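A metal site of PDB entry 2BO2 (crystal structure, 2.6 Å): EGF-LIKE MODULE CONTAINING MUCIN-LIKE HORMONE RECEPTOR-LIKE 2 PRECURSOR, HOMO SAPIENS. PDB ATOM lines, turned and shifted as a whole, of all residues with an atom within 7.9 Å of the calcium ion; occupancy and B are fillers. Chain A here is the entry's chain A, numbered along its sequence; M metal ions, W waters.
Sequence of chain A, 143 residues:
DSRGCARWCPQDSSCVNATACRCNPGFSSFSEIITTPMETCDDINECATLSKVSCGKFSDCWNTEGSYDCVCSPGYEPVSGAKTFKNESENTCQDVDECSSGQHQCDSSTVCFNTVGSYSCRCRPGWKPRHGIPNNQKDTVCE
SG of Cys 47 lies within hydrogen-bond range of N of Asn 63 (3.4 Å).
N of Tyr 68 is in hydrogen-bond range of OG1 of Thr 64, at 3.2 Å.
The side-chain hydroxyl (OG1) of Thr 64 sits close to the backbone NH (N) of Ser 67.
The side-chain carboxylate (OD1) of Asp 43 lies close to the backbone NH (N) of Gly 66 (3.0 Å).
The backbone NH (N) of Ile 44 lies within hydrogen-bond range of the backbone carbonyl oxygen (O) of Gly 26, at 2.8 Å.
Six residues have an atom within 4 Å of the calcium ion: Asp 43, Ile 44, Glu 46, Asn 63, Thr 64 and Ser 67.
The calcium ion is bound by water W1, the side-chain amide oxygen of Asn 63, the backbone carbonyl oxygen of Ile 44, the side-chain carboxylate of Asp 43, the backbone carbonyl oxygen of Ser 67, the backbone carbonyl oxygen of Thr 64 and the side-chain carboxylate of Glu 46.
Water W1 lies within hydrogen-bond range of the side-chain carboxylate (OE2) of Glu 46 (2.5 Å), the backbone NH (N) of Ser 67 (3.0 Å) and the backbone carbonyl oxygen (O) of Gly 26 (3.1 Å).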
ATOM      1  N   GLY A  26     -10.555   1.609 -12.895  1.00  0.00           N
ATOM      2  CA  GLY A  26     -10.084   2.866 -13.457  1.00  0.00           C
ATOM      3  C   GLY A  26     -11.191   3.911 -13.499  1.00  0.00           C
ATOM      4  O   GLY A  26     -10.942   5.083 -13.800  1.00  0.00           O
ATOM      5  N   PHE A  27     -12.412   3.486 -13.189  1.00  0.00           N
ATOM      6  CA  PHE A  27     -13.557   4.390 -13.171  1.00  0.00           C
ATOM      7  C   PHE A  27     -14.262   4.366 -11.829  1.00  0.00           C
ATOM      8  O   PHE A  27     -14.094   3.426 -11.043  1.00  0.00           O
ATOM      9  CB  PHE A  27     -14.548   4.020 -14.277  1.00  0.00           C
ATOM     10  CG  PHE A  27     -13.963   4.068 -15.665  1.00  0.00           C
ATOM     11  CD1 PHE A  27     -13.364   2.947 -16.210  1.00  0.00           C
ATOM     12  CD2 PHE A  27     -14.020   5.227 -16.417  1.00  0.00           C
ATOM     13  CE1 PHE A  27     -12.828   2.983 -17.477  1.00  0.00           C
ATOM     14  CE2 PHE A  27     -13.474   5.273 -17.690  1.00  0.00           C
ATOM     15  CZ  PHE A  27     -12.872   4.150 -18.212  1.00  0.00           C
ATOM     16  N   ASP A  42     -17.259   7.359 -14.095  1.00  0.00           N
ATOM     17  CA  ASP A  42     -16.303   8.370 -14.520  1.00  0.00           C
ATOM     18  C   ASP A  42     -14.852   8.002 -14.243  1.00  0.00           C
ATOM     19  O   ASP A  42     -14.533   7.377 -13.239  1.00  0.00           O
ATOM     20  CB  ASP A  42     -16.648   9.725 -13.918  1.00  0.00           C
ATOM     21  CG  ASP A  42     -18.061  10.163 -14.251  1.00  0.00           C
ATOM     22  OD1 ASP A  42     -18.300  10.569 -15.417  1.00  0.00           O
ATOM     23  OD2 ASP A  42     -18.942  10.043 -13.378  1.00  0.00           O
ATOM     24  N   ASP A  43     -13.979   8.397 -15.161  1.00  0.00           N
ATOM     25  CA  ASP A  43     -12.559   8.094 -15.064  1.00  0.00           C
ATOM     26  C   ASP A  43     -11.913   8.628 -13.798  1.00  0.00           C
ATOM     27  O   ASP A  43     -12.064   9.800 -13.460  1.00  0.00           O
ATOM     28  CB  ASP A  43     -11.810   8.621 -16.298  1.00  0.00           C
ATOM     29  CG  ASP A  43     -10.349   8.877 -16.033  1.00  0.00           C
ATOM     30  OD1 ASP A  43      -9.574   7.904 -15.990  1.00  0.00           O
ATOM     31  OD2 ASP A  43      -9.966  10.049 -15.897  1.00  0.00           O
ATOM     32  N   ILE A  44     -11.157   7.770 -13.130  1.00  0.00           N
ATOM     33  CA  ILE A  44     -10.413   8.169 -11.940  1.00  0.00           C
ATOM     34  C   ILE A  44      -9.126   8.859 -12.400  1.00  0.00           C
ATOM     35  O   ILE A  44      -8.469   8.400 -13.334  1.00  0.00           O
ATOM     36  CB  ILE A  44     -10.033   6.943 -11.083  1.00  0.00           C
ATOM     37  CG1 ILE A  44     -11.260   6.364 -10.380  1.00  0.00           C
ATOM     38  CG2 ILE A  44      -8.963   7.312 -10.073  1.00  0.00           C
ATOM     39  CD1 ILE A  44     -11.005   5.012  -9.735  1.00  0.00           C
ATOM     40  N   ASN A  45      -8.781   9.975 -11.770  1.00  0.00           N
ATOM     41  CA  ASN A  45      -7.543  10.671 -12.094  1.00  0.00           C
ATOM     42  C   ASN A  45      -6.465  10.265 -11.103  1.00  0.00           C
ATOM     43  O   ASN A  45      -6.309  10.880 -10.054  1.00  0.00           O
ATOM     44  CB  ASN A  45      -7.725  12.196 -12.060  1.00  0.00           C
ATOM     45  CG  ASN A  45      -6.475  12.939 -12.523  1.00  0.00           C
ATOM     46  OD1 ASN A  45      -5.384  12.374 -12.569  1.00  0.00           O
ATOM     47  ND2 ASN A  45      -6.636  14.213 -12.848  1.00  0.00           N
ATOM     48  N   GLU A  46      -5.740   9.200 -11.446  1.00  0.00           N
ATOM     49  CA  GLU A  46      -4.709   8.655 -10.576  1.00  0.00           C
ATOM     50  C   GLU A  46      -3.578   9.636 -10.288  1.00  0.00           C
ATOM     51  O   GLU A  46      -2.824   9.444  -9.331  1.00  0.00           O
ATOM     52  CB  GLU A  46      -4.159   7.360 -11.158  1.00  0.00           C
ATOM     53  CG  GLU A  46      -5.148   6.215 -11.124  1.00  0.00           C
ATOM     54  CD  GLU A  46      -5.929   6.086 -12.400  1.00  0.00           C
ATOM     55  OE1 GLU A  46      -5.906   7.029 -13.213  1.00  0.00           O
ATOM     56  OE2 GLU A  46      -6.563   5.022 -12.614  1.00  0.00           O
ATOM     57  N   CYS A  47      -3.449  10.670 -11.115  1.00  0.00           N
ATOM     58  CA  CYS A  47      -2.365  11.633 -10.957  1.00  0.00           C
ATOM     59  C   CYS A  47      -2.666  12.781  -9.991  1.00  0.00           C
ATOM     60  O   CYS A  47      -1.783  13.572  -9.672  1.00  0.00           O
ATOM     61  CB  CYS A  47      -1.932  12.188 -12.317  1.00  0.00           C
ATOM     62  SG  CYS A  47      -1.411  10.912 -13.497  1.00  0.00           S
ATOM     63  N   TRP A  62       0.836  11.152 -16.018  1.00  0.00           N
ATOM     64  CA  TRP A  62      -0.097  11.577 -17.050  1.00  0.00           C
ATOM     65  C   TRP A  62      -1.369  10.748 -16.967  1.00  0.00           C
ATOM     66  O   TRP A  62      -1.328   9.524 -17.096  1.00  0.00           O
ATOM     67  CB  TRP A  62       0.534  11.450 -18.432  1.00  0.00           C
ATOM     68  CG  TRP A  62       1.475  12.568 -18.783  1.00  0.00           C
ATOM     69  CD1 TRP A  62       2.792  12.672 -18.434  1.00  0.00           C
ATOM     70  CD2 TRP A  62       1.171  13.742 -19.552  1.00  0.00           C
ATOM     71  NE1 TRP A  62       3.330  13.838 -18.933  1.00  0.00           N
ATOM     72  CE2 TRP A  62       2.359  14.509 -19.643  1.00  0.00           C
ATOM     73  CE3 TRP A  62       0.017  14.214 -20.193  1.00  0.00           C
ATOM     74  CZ2 TRP A  62       2.419  15.703 -20.339  1.00  0.00           C
ATOM     75  CZ3 TRP A  62       0.091  15.407 -20.886  1.00  0.00           C
ATOM     76  CH2 TRP A  62       1.278  16.141 -20.944  1.00  0.00           C
ATOM     77  N   ASN A  63      -2.489  11.414 -16.713  1.00  0.00           N
ATOM     78  CA  ASN A  63      -3.760  10.733 -16.587  1.00  0.00           C
ATOM     79  C   ASN A  63      -4.375  10.422 -17.946  1.00  0.00           C
ATOM     80  O   ASN A  63      -4.257  11.193 -18.888  1.00  0.00           O
ATOM     81  CB  ASN A  63      -4.729  11.560 -15.750  1.00  0.00           C
ATOM     82  CG  ASN A  63      -6.017  10.843 -15.492  1.00  0.00           C
ATOM     83  OD1 ASN A  63      -6.018   9.689 -15.058  1.00  0.00           O
ATOM     84  ND2 ASN A  63      -7.141  11.511 -15.769  1.00  0.00           N
ATOM     85  N   THR A  64      -5.052   9.274 -18.027  1.00  0.00           N
ATOM     86  CA  THR A  64      -5.709   8.839 -19.248  1.00  0.00           C
ATOM     87  C   THR A  64      -7.080   8.285 -18.896  1.00  0.00           C
ATOM     88  O   THR A  64      -7.319   7.886 -17.755  1.00  0.00           O
ATOM     89  CB  THR A  64      -4.884   7.757 -19.976  1.00  0.00           C
ATOM     90  OG1 THR A  64      -4.746   6.605 -19.133  1.00  0.00           O
ATOM     91  CG2 THR A  64      -3.489   8.288 -20.311  1.00  0.00           C
ATOM     92  N   GLU A  65      -7.989   8.280 -19.864  1.00  0.00           N
ATOM     93  CA  GLU A  65      -9.332   7.761 -19.628  1.00  0.00           C
ATOM     94  C   GLU A  65      -9.294   6.264 -19.404  1.00  0.00           C
ATOM     95  O   GLU A  65      -9.215   5.489 -20.359  1.00  0.00           O
ATOM     96  CB  GLU A  65     -10.245   8.082 -20.811  1.00  0.00           C
ATOM     97  CG  GLU A  65     -10.844   9.476 -20.778  1.00  0.00           C
ATOM     98  CD  GLU A  65     -12.234   9.503 -20.187  1.00  0.00           C
ATOM     99  OE1 GLU A  65     -13.198   9.188 -20.921  1.00  0.00           O
ATOM    100  OE2 GLU A  65     -12.374   9.846 -18.997  1.00  0.00           O
ATOM    101  N   GLY A  66      -9.344   5.859 -18.140  1.00  0.00           N
ATOM    102  CA  GLY A  66      -9.345   4.449 -17.790  1.00  0.00           C
ATOM    103  C   GLY A  66      -8.018   3.983 -17.199  1.00  0.00           C
ATOM    104  O   GLY A  66      -7.904   2.839 -16.761  1.00  0.00           O
ATOM    105  N   SER A  67      -7.035   4.874 -17.175  1.00  0.00           N
ATOM    106  CA  SER A  67      -5.724   4.533 -16.631  1.00  0.00           C
ATOM    107  C   SER A  67      -4.857   5.772 -16.365  1.00  0.00           C
ATOM    108  O   SER A  67      -5.371   6.878 -16.195  1.00  0.00           O
ATOM    109  CB  SER A  67      -4.991   3.574 -17.563  1.00  0.00           C
ATOM    110  OG  SER A  67      -4.106   2.730 -16.837  1.00  0.00           O
ATOM    111  N   TYR A  68      -3.552   5.555 -16.347  1.00  0.00           N
ATOM    112  CA  TYR A  68      -2.572   6.626 -16.136  1.00  0.00           C
ATOM    113  C   TYR A  68      -1.202   6.085 -16.531  1.00  0.00           C
ATOM    114  O   TYR A  68      -1.025   4.868 -16.645  1.00  0.00           O
ATOM    115  CB  TYR A  68      -2.548   7.026 -14.659  1.00  0.00           C
ATOM    116  CG  TYR A  68      -1.721   6.089 -13.804  1.00  0.00           C
ATOM    117  CD1 TYR A  68      -0.361   6.300 -13.622  1.00  0.00           C
ATOM    118  CD2 TYR A  68      -2.296   4.962 -13.223  1.00  0.00           C
ATOM    119  CE1 TYR A  68       0.409   5.425 -12.866  1.00  0.00           C
ATOM    120  CE2 TYR A  68      -1.541   4.078 -12.470  1.00  0.00           C
ATOM    121  CZ  TYR A  68      -0.200   4.320 -12.282  1.00  0.00           C
ATOM    122  OH  TYR A  68       0.548   3.447 -11.523  1.00  0.00           O
ATOM    123  N   ASP A  69      -0.232   6.969 -16.710  1.00  0.00           N
ATOM    124  CA  ASP A  69       1.115   6.549 -17.060  1.00  0.00           C
ATOM    125  C   ASP A  69       2.170   7.468 -16.463  1.00  0.00           C
ATOM    126  O   ASP A  69       1.973   8.679 -16.360  1.00  0.00           O
ATOM    127  CB  ASP A  69       1.297   6.525 -18.587  1.00  0.00           C
ATOM    128  CG  ASP A  69       0.578   5.356 -19.250  1.00  0.00           C
ATOM    129  OD1 ASP A  69       1.018   4.196 -19.075  1.00  0.00           O
ATOM    130  OD2 ASP A  69      -0.390   5.605 -19.993  1.00  0.00           O
HETATM  131 CA    CA M   1      -7.335   7.857 -15.286  1.00  0.00          CA
HETATM  132  O   HOH W   1      -7.995   5.870 -14.508  1.00  0.00           O
